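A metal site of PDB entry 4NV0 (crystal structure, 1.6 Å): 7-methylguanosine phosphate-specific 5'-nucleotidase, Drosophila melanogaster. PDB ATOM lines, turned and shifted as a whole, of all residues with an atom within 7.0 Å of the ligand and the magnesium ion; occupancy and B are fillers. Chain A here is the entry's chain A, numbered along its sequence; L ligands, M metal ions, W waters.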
ATOM      1  N   SER A  54     -27.734  -4.141 -27.114  1.00  0.00           N
ATOM      2  CA  SER A  54     -26.749  -4.314 -26.043  1.00  0.00           C
ATOM      3  C   SER A  54     -27.394  -4.400 -24.670  1.00  0.00           C
ATOM      4  O   SER A  54     -28.370  -3.684 -24.384  1.00  0.00           O
ATOM      5  CB  SER A  54     -25.826  -3.093 -26.040  1.00  0.00           C
ATOM      6  OG  SER A  54     -24.812  -3.185 -25.033  1.00  0.00           O
ATOM      7  N   ASP A  55     -26.818  -5.231 -23.827  1.00  0.00           N
ATOM      8  CA  ASP A  55     -27.134  -5.308 -22.403  1.00  0.00           C
ATOM      9  C   ASP A  55     -26.572  -4.019 -21.758  1.00  0.00           C
ATOM     10  O   ASP A  55     -25.726  -3.339 -22.353  1.00  0.00           O
ATOM     11  CB  ASP A  55     -26.369  -6.491 -21.845  1.00  0.00           C
ATOM     12  CG  ASP A  55     -26.521  -6.636 -20.392  1.00  0.00           C
ATOM     13  OD1 ASP A  55     -27.682  -6.674 -20.015  1.00  0.00           O
ATOM     14  OD2 ASP A  55     -25.527  -6.748 -19.663  1.00  0.00           O
ATOM     15  N   PHE A  56     -27.047  -3.666 -20.561  1.00  0.00           N
ATOM     16  CA  PHE A  56     -26.470  -2.530 -19.835  1.00  0.00           C
ATOM     17  C   PHE A  56     -25.523  -2.980 -18.692  1.00  0.00           C
ATOM     18  O   PHE A  56     -24.320  -2.708 -18.739  1.00  0.00           O
ATOM     19  CB  PHE A  56     -27.591  -1.652 -19.233  1.00  0.00           C
ATOM     20  CG  PHE A  56     -27.051  -0.526 -18.410  1.00  0.00           C
ATOM     21  CD1 PHE A  56     -26.504   0.599 -19.029  1.00  0.00           C
ATOM     22  CD2 PHE A  56     -27.032  -0.617 -17.026  1.00  0.00           C
ATOM     23  CE1 PHE A  56     -25.993   1.656 -18.224  1.00  0.00           C
ATOM     24  CE2 PHE A  56     -26.503   0.406 -16.251  1.00  0.00           C
ATOM     25  CZ  PHE A  56     -25.992   1.536 -16.864  1.00  0.00           C
ATOM     26  N   ASP A  57     -26.051  -3.662 -17.677  1.00  0.00           N
ATOM     27  CA  ASP A  57     -25.249  -3.897 -16.468  1.00  0.00           C
ATOM     28  C   ASP A  57     -24.066  -4.817 -16.763  1.00  0.00           C
ATOM     29  O   ASP A  57     -24.240  -5.964 -17.195  1.00  0.00           O
ATOM     30  CB  ASP A  57     -26.119  -4.521 -15.366  1.00  0.00           C
ATOM     31  CG  ASP A  57     -27.121  -3.525 -14.757  1.00  0.00           C
ATOM     32  OD1 ASP A  57     -26.656  -2.484 -14.243  1.00  0.00           O
ATOM     33  OD2 ASP A  57     -28.353  -3.770 -14.792  1.00  0.00           O
ATOM     34  N   TYR A  58     -22.860  -4.300 -16.536  1.00  0.00           N
ATOM     35  CA  TYR A  58     -21.602  -5.015 -16.750  1.00  0.00           C
ATOM     36  C   TYR A  58     -21.265  -5.293 -18.224  1.00  0.00           C
ATOM     37  O   TYR A  58     -20.336  -6.037 -18.539  1.00  0.00           O
ATOM     38  CB  TYR A  58     -21.514  -6.286 -15.851  1.00  0.00           C
ATOM     39  CG  TYR A  58     -21.831  -5.896 -14.422  1.00  0.00           C
ATOM     40  CD1 TYR A  58     -21.016  -5.015 -13.727  1.00  0.00           C
ATOM     41  CD2 TYR A  58     -23.016  -6.303 -13.829  1.00  0.00           C
ATOM     42  CE1 TYR A  58     -21.333  -4.618 -12.434  1.00  0.00           C
ATOM     43  CE2 TYR A  58     -23.355  -5.901 -12.528  1.00  0.00           C
ATOM     44  CZ  TYR A  58     -22.512  -5.048 -11.838  1.00  0.00           C
ATOM     45  OH  TYR A  58     -22.845  -4.640 -10.533  1.00  0.00           O
ATOM     46  N   THR A  59     -22.034  -4.687 -19.134  1.00  0.00           N
ATOM     47  CA  THR A  59     -21.669  -4.605 -20.548  1.00  0.00           C
ATOM     48  C   THR A  59     -21.308  -3.173 -20.863  1.00  0.00           C
ATOM     49  O   THR A  59     -20.199  -2.866 -21.289  1.00  0.00           O
ATOM     50  CB  THR A  59     -22.837  -5.085 -21.429  1.00  0.00           C
ATOM     51  OG1 THR A  59     -23.078  -6.466 -21.129  1.00  0.00           O
ATOM     52  CG2 THR A  59     -22.506  -4.939 -22.924  1.00  0.00           C
ATOM     53  N   ILE A  60     -22.231  -2.240 -20.624  1.00  0.00           N
ATOM     54  CA  ILE A  60     -21.943  -0.842 -20.814  1.00  0.00           C
ATOM     55  C   ILE A  60     -21.206  -0.316 -19.611  1.00  0.00           C
ATOM     56  O   ILE A  60     -20.218   0.395 -19.753  1.00  0.00           O
ATOM     57  CB  ILE A  60     -23.221  -0.048 -21.155  1.00  0.00           C
ATOM     58  CG1 ILE A  60     -23.684  -0.457 -22.549  1.00  0.00           C
ATOM     59  CG2 ILE A  60     -22.949   1.484 -21.122  1.00  0.00           C
ATOM     60  CD1 ILE A  60     -25.087   0.058 -22.908  1.00  0.00           C
ATOM     61  N   SER A  74     -28.011  -1.536 -11.982  1.00  0.00           N
ATOM     62  CA  SER A  74     -29.114  -0.577 -12.076  1.00  0.00           C
ATOM     63  C   SER A  74     -30.074  -0.657 -10.843  1.00  0.00           C
ATOM     64  O   SER A  74     -30.517   0.389 -10.256  1.00  0.00           O
ATOM     65  CB  SER A  74     -29.845  -0.808 -13.406  1.00  0.00           C
ATOM     66  OG  SER A  74     -30.205  -2.175 -13.603  1.00  0.00           O
ATOM     67  N   TRP A 121     -38.777 -11.037  -9.719  1.00  0.00           N
ATOM     68  CA  TRP A 121     -39.124  -9.724 -10.255  1.00  0.00           C
ATOM     69  C   TRP A 121     -40.516  -9.282  -9.782  1.00  0.00           C
ATOM     70  O   TRP A 121     -40.754  -8.092  -9.537  1.00  0.00           O
ATOM     71  CB  TRP A 121     -39.002  -9.726 -11.783  1.00  0.00           C
ATOM     72  CG  TRP A 121     -37.670  -9.248 -12.337  1.00  0.00           C
ATOM     73  CD1 TRP A 121     -37.430  -8.022 -12.935  1.00  0.00           C
ATOM     74  CD2 TRP A 121     -36.416  -9.964 -12.392  1.00  0.00           C
ATOM     75  NE1 TRP A 121     -36.121  -7.934 -13.323  1.00  0.00           N
ATOM     76  CE2 TRP A 121     -35.476  -9.112 -13.031  1.00  0.00           C
ATOM     77  CE3 TRP A 121     -35.998 -11.232 -11.967  1.00  0.00           C
ATOM     78  CZ2 TRP A 121     -34.145  -9.483 -13.246  1.00  0.00           C
ATOM     79  CZ3 TRP A 121     -34.676 -11.612 -12.177  1.00  0.00           C
ATOM     80  CH2 TRP A 121     -33.762 -10.729 -12.821  1.00  0.00           C
ATOM     81  N   VAL A 169     -30.748  -0.541 -25.897  1.00  0.00           N
ATOM     82  CA  VAL A 169     -30.201  -1.050 -24.653  1.00  0.00           C
ATOM     83  C   VAL A 169     -31.333  -1.866 -24.015  1.00  0.00           C
ATOM     84  O   VAL A 169     -32.352  -1.320 -23.643  1.00  0.00           O
ATOM     85  CB  VAL A 169     -29.752   0.101 -23.753  1.00  0.00           C
ATOM     86  CG1 VAL A 169     -29.258  -0.434 -22.409  1.00  0.00           C
ATOM     87  CG2 VAL A 169     -28.661   0.942 -24.443  1.00  0.00           C
ATOM     88  N   PHE A 170     -31.151  -3.186 -23.959  1.00  0.00           N
ATOM     89  CA  PHE A 170     -32.175  -4.168 -23.582  1.00  0.00           C
ATOM     90  C   PHE A 170     -31.687  -4.733 -22.260  1.00  0.00           C
ATOM     91  O   PHE A 170     -30.682  -5.472 -22.207  1.00  0.00           O
ATOM     92  CB  PHE A 170     -32.165  -5.242 -24.684  1.00  0.00           C
ATOM     93  CG  PHE A 170     -33.343  -6.193 -24.676  1.00  0.00           C
ATOM     94  CD1 PHE A 170     -34.313  -6.174 -23.700  1.00  0.00           C
ATOM     95  CD2 PHE A 170     -33.421  -7.158 -25.682  1.00  0.00           C
ATOM     96  CE1 PHE A 170     -35.353  -7.095 -23.732  1.00  0.00           C
ATOM     97  CE2 PHE A 170     -34.460  -8.076 -25.724  1.00  0.00           C
ATOM     98  CZ  PHE A 170     -35.422  -8.061 -24.759  1.00  0.00           C
ATOM     99  N   SER A 171     -32.390  -4.421 -21.171  1.00  0.00           N
ATOM    100  CA  SER A 171     -31.869  -4.660 -19.822  1.00  0.00           C
ATOM    101  C   SER A 171     -32.943  -5.261 -18.909  1.00  0.00           C
ATOM    102  O   SER A 171     -34.033  -4.710 -18.848  1.00  0.00           O
ATOM    103  CB  SER A 171     -31.418  -3.330 -19.236  1.00  0.00           C
ATOM    104  OG  SER A 171     -31.076  -3.507 -17.876  1.00  0.00           O
ATOM    105  N   ALA A 172     -32.617  -6.325 -18.178  1.00  0.00           N
ATOM    106  CA  ALA A 172     -33.540  -6.896 -17.218  1.00  0.00           C
ATOM    107  C   ALA A 172     -33.454  -6.160 -15.879  1.00  0.00           C
ATOM    108  O   ALA A 172     -34.012  -6.600 -14.875  1.00  0.00           O
ATOM    109  CB  ALA A 172     -33.217  -8.396 -17.016  1.00  0.00           C
ATOM    110  N   GLY A 173     -32.723  -5.046 -15.871  1.00  0.00           N
ATOM    111  CA  GLY A 173     -32.502  -4.286 -14.650  1.00  0.00           C
ATOM    112  C   GLY A 173     -33.586  -3.258 -14.408  1.00  0.00           C
ATOM    113  O   GLY A 173     -34.716  -3.408 -14.863  1.00  0.00           O
ATOM    114  N   LEU A 174     -33.222  -2.189 -13.711  1.00  0.00           N
ATOM    115  CA  LEU A 174     -34.164  -1.137 -13.360  1.00  0.00           C
ATOM    116  C   LEU A 174     -33.947   0.001 -14.366  1.00  0.00           C
ATOM    117  O   LEU A 174     -32.899   0.692 -14.355  1.00  0.00           O
ATOM    118  CB  LEU A 174     -33.920  -0.730 -11.899  1.00  0.00           C
ATOM    119  CG  LEU A 174     -35.007  -0.023 -11.070  1.00  0.00           C
ATOM    120  CD1 LEU A 174     -35.049   1.446 -11.371  1.00  0.00           C
ATOM    121  CD2 LEU A 174     -36.394  -0.660 -11.230  1.00  0.00           C
ATOM    122  N   VAL A 178     -30.841   2.832 -15.553  1.00  0.00           N
ATOM    123  CA  VAL A 178     -30.146   2.740 -16.837  1.00  0.00           C
ATOM    124  C   VAL A 178     -30.217   4.066 -17.608  1.00  0.00           C
ATOM    125  O   VAL A 178     -29.187   4.602 -18.100  1.00  0.00           O
ATOM    126  CB  VAL A 178     -30.792   1.629 -17.706  1.00  0.00           C
ATOM    127  CG1 VAL A 178     -30.152   1.601 -19.118  1.00  0.00           C
ATOM    128  CG2 VAL A 178     -30.621   0.233 -17.037  1.00  0.00           C
ATOM    129  N   SER A 196     -36.654  -1.966 -20.739  1.00  0.00           N
ATOM    130  CA  SER A 196     -36.246  -2.467 -19.432  1.00  0.00           C
ATOM    131  C   SER A 196     -37.449  -2.444 -18.518  1.00  0.00           C
ATOM    132  O   SER A 196     -38.568  -2.309 -19.006  1.00  0.00           O
ATOM    133  CB  SER A 196     -35.130  -1.580 -18.863  1.00  0.00           C
ATOM    134  OG  SER A 196     -34.576  -2.144 -17.679  1.00  0.00           O
ATOM    135  N   ILE A 214     -39.243  -8.017 -17.608  1.00  0.00           N
ATOM    136  CA  ILE A 214     -38.076  -8.475 -18.331  1.00  0.00           C
ATOM    137  C   ILE A 214     -37.122  -8.988 -17.293  1.00  0.00           C
ATOM    138  O   ILE A 214     -36.668  -8.234 -16.449  1.00  0.00           O
ATOM    139  CB  ILE A 214     -37.458  -7.327 -19.111  1.00  0.00           C
ATOM    140  CG1 ILE A 214     -38.478  -6.811 -20.139  1.00  0.00           C
ATOM    141  CG2 ILE A 214     -36.183  -7.831 -19.851  1.00  0.00           C
ATOM    142  CD1 ILE A 214     -38.049  -5.579 -20.839  1.00  0.00           C
ATOM    143  N   HIS A 215     -36.854 -10.293 -17.324  1.00  0.00           N
ATOM    144  CA  HIS A 215     -35.905 -10.856 -16.357  1.00  0.00           C
ATOM    145  C   HIS A 215     -34.735 -11.473 -17.142  1.00  0.00           C
ATOM    146  O   HIS A 215     -34.665 -11.374 -18.368  1.00  0.00           O
ATOM    147  CB  HIS A 215     -36.569 -11.887 -15.439  1.00  0.00           C
ATOM    148  CG  HIS A 215     -37.284 -12.973 -16.184  1.00  0.00           C
ATOM    149  ND1 HIS A 215     -36.615 -13.997 -16.830  1.00  0.00           N
ATOM    150  CD2 HIS A 215     -38.602 -13.194 -16.387  1.00  0.00           C
ATOM    151  CE1 HIS A 215     -37.498 -14.776 -17.428  1.00  0.00           C
ATOM    152  NE2 HIS A 215     -38.712 -14.323 -17.165  1.00  0.00           N
ATOM    153  N   THR A 216     -33.836 -12.135 -16.420  1.00  0.00           N
ATOM    154  CA  THR A 216     -32.565 -12.556 -16.983  1.00  0.00           C
ATOM    155  C   THR A 216     -32.759 -13.517 -18.116  1.00  0.00           C
ATOM    156  O   THR A 216     -31.942 -13.555 -19.040  1.00  0.00           O
ATOM    157  CB  THR A 216     -31.684 -13.241 -15.941  1.00  0.00           C
ATOM    158  OG1 THR A 216     -31.543 -12.375 -14.816  1.00  0.00           O
ATOM    159  CG2 THR A 216     -30.278 -13.556 -16.508  1.00  0.00           C
ATOM    160  N   LYS A 219     -35.008 -12.273 -22.201  1.00  0.00           N
ATOM    161  CA  LYS A 219     -34.569 -11.201 -23.092  1.00  0.00           C
ATOM    162  C   LYS A 219     -34.447 -11.761 -24.506  1.00  0.00           C
ATOM    163  O   LYS A 219     -33.356 -11.940 -25.042  1.00  0.00           O
ATOM    164  CB  LYS A 219     -33.214 -10.608 -22.663  1.00  0.00           C
ATOM    165  CG  LYS A 219     -33.219  -9.970 -21.277  1.00  0.00           C
ATOM    166  CD  LYS A 219     -31.806  -9.607 -20.828  1.00  0.00           C
ATOM    167  CE  LYS A 219     -31.302  -8.402 -21.600  1.00  0.00           C
ATOM    168  NZ  LYS A 219     -29.915  -8.007 -21.156  1.00  0.00           N
ATOM    169  N   GLY A 244     -23.206  -8.479 -24.831  1.00  0.00           N
ATOM    170  CA  GLY A 244     -23.574  -8.647 -23.425  1.00  0.00           C
ATOM    171  C   GLY A 244     -22.518  -9.362 -22.628  1.00  0.00           C
ATOM    172  O   GLY A 244     -21.532  -9.783 -23.200  1.00  0.00           O
ATOM    173  N   ASP A 245     -22.754  -9.512 -21.320  1.00  0.00           N
ATOM    174  CA  ASP A 245     -21.770 -10.179 -20.467  1.00  0.00           C
ATOM    175  C   ASP A 245     -22.277 -11.521 -19.934  1.00  0.00           C
ATOM    176  O   ASP A 245     -21.531 -12.243 -19.259  1.00  0.00           O
ATOM    177  CB  ASP A 245     -21.388  -9.297 -19.273  1.00  0.00           C
ATOM    178  CG  ASP A 245     -22.570  -9.060 -18.306  1.00  0.00           C
ATOM    179  OD1 ASP A 245     -23.566  -8.404 -18.695  1.00  0.00           O
ATOM    180  OD2 ASP A 245     -22.488  -9.511 -17.137  1.00  0.00           O
ATOM    181  N   SER A 246     -23.538 -11.853 -20.249  1.00  0.00           N
ATOM    182  CA  SER A 246     -24.184 -13.078 -19.712  1.00  0.00           C
ATOM    183  C   SER A 246     -24.595 -13.982 -20.866  1.00  0.00           C
ATOM    184  O   SER A 246     -24.915 -13.501 -21.928  1.00  0.00           O
ATOM    185  CB  SER A 246     -25.472 -12.706 -18.933  1.00  0.00           C
ATOM    186  OG  SER A 246     -25.216 -11.865 -17.818  1.00  0.00           O
ATOM    187  N   ASP A 249     -27.797 -13.147 -22.628  1.00  0.00           N
ATOM    188  CA  ASP A 249     -27.862 -11.981 -23.525  1.00  0.00           C
ATOM    189  C   ASP A 249     -27.742 -12.376 -25.013  1.00  0.00           C
ATOM    190  O   ASP A 249     -28.025 -11.583 -25.912  1.00  0.00           O
ATOM    191  CB  ASP A 249     -26.744 -10.998 -23.202  1.00  0.00           C
ATOM    192  CG  ASP A 249     -26.901 -10.337 -21.846  1.00  0.00           C
ATOM    193  OD1 ASP A 249     -28.049 -10.157 -21.405  1.00  0.00           O
ATOM    194  OD2 ASP A 249     -25.856 -10.013 -21.220  1.00  0.00           O
ATOM    195  N   MET A 252     -30.850 -11.902 -27.529  1.00  0.00           N
ATOM    196  CA  MET A 252     -31.606 -10.660 -27.478  1.00  0.00           C
ATOM    197  C   MET A 252     -32.258 -10.284 -28.817  1.00  0.00           C
ATOM    198  O   MET A 252     -33.309  -9.653 -28.839  1.00  0.00           O
ATOM    199  CB  MET A 252     -30.721  -9.525 -26.965  1.00  0.00           C
ATOM    200  CG  MET A 252     -30.510  -9.616 -25.440  1.00  0.00           C
ATOM    201  SD  MET A 252     -29.645  -8.146 -24.840  1.00  0.00           S
ATOM    202  CE  MET A 252     -28.063  -8.237 -25.719  1.00  0.00           C
HETATM  203  F1  LIG L   1     -28.573  -4.548 -18.242  1.00  0.00           F
HETATM  204 MG1  LIG L   1     -28.599  -6.424 -17.949  1.00  0.00          MG
HETATM  205  F2  LIG L   1     -30.050  -7.533 -18.330  1.00  0.00           F
HETATM  206  F3  LIG L   1     -26.964  -7.077 -17.123  1.00  0.00           F
HETATM  207 MG    MG M   1     -25.268  -7.677 -17.830  1.00  0.00          MG
HETATM  208  O   HOH W   1     -26.267  -9.502 -18.667  1.00  0.00           O
HETATM  209  O   HOH W   2     -29.641  -5.802 -15.889  1.00  0.00           O
HETATM  210  O   HOH W   3     -29.011  -9.830 -17.996  1.00  0.00           O
HETATM  211  O   HOH W   4     -24.785  -8.718 -16.036  1.00  0.00           O
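Water W1 lies within hydrogen-bond range of the side-chain carboxylate (OD2) of Asp 249 (2.6 Å) and the side-chain hydroxyl (OG) of Ser 246 (2.7 Å). Water W2 lies within hydrogen-bond range of the side-chain carboxylate (OD2) of Asp 57 (2.6 Å), the backbone NH (N) of Gly 173 (3.2 Å) and the side-chain hydroxyl (OG) of Ser 171 (3.4 Å).
Along chain A the residues within 4 Å of the ligand span positions 55 to 245. The nearest printed residue that does not touch the ligand is Gly 173 (4.4 Å).
Within 4 Å of the magnesium ion: Asp 55, Asp 57 and Asp 245. The nearest printed residue that does not touch the magnesium ion is Thr 59 (4.1 Å).
The magnesium ion is bound by F3 of the ligand (1.9 Å), OD1 of Asp 245 (2.0 Å), OD2 of Asp 55 (2.1 Å), O of Asp 57 (2.1 Å), water W4 (2.1 Å) and water W1 (2.2 Å).
The side-chain hydroxyl (OG1) of Thr 59 sits at hydrogen-bond distance from the backbone NH (N) of Asp 245 (3.1 Å). The side-chain carboxylate (OD1) of Asp 55 lies close to the side-chain amino group (NZ) of Lys 219, at 2.8 Å. OD2 of Asp 55 sits close to OG1 of Thr 59 (2.9 Å). OG of Ser 74 lies within hydrogen-bond range of OD2 of Asp 57. The side-chain hydroxyl (OG) of Ser 171 sits at hydrogen-bond distance from the backbone NH (N) of Gly 173 (3.0 Å). The backbone carbonyl oxygen of Ala 172 is in hydrogen-bond range of the indole nitrogen of Trp 121, 2.9 Å away. The side-chain amino group (NZ) of Lys 219 is in salt-bridge range of the side-chain carboxylate (OD1) of Asp 249 (2.9 Å). NZ of Lys 219 sits close to SD of Met 252 (3.7 Å).
The side-chain carboxylate of Asp 55 is bound to a magnesium atom (MG1) of the ligand, at 2.3 Å. N of Asp 57 is in hydrogen-bond range of F1 of the ligand. OG of Ser 171 sits at hydrogen-bond distance from F1 of the ligand (2.7 Å). The backbone NH of Ala 172 lies within hydrogen-bond range of a fluorine (F2) of the ligand (2.8 Å). A fluorine (F2) of the ligand sits at hydrogen-bond distance from the side-chain amino group (NZ) of Lys 219 (2.9 Å). The backbone NH (N) of Phe 56 lies within hydrogen-bond range of a fluorine (F1) of the ligand (2.9 Å).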
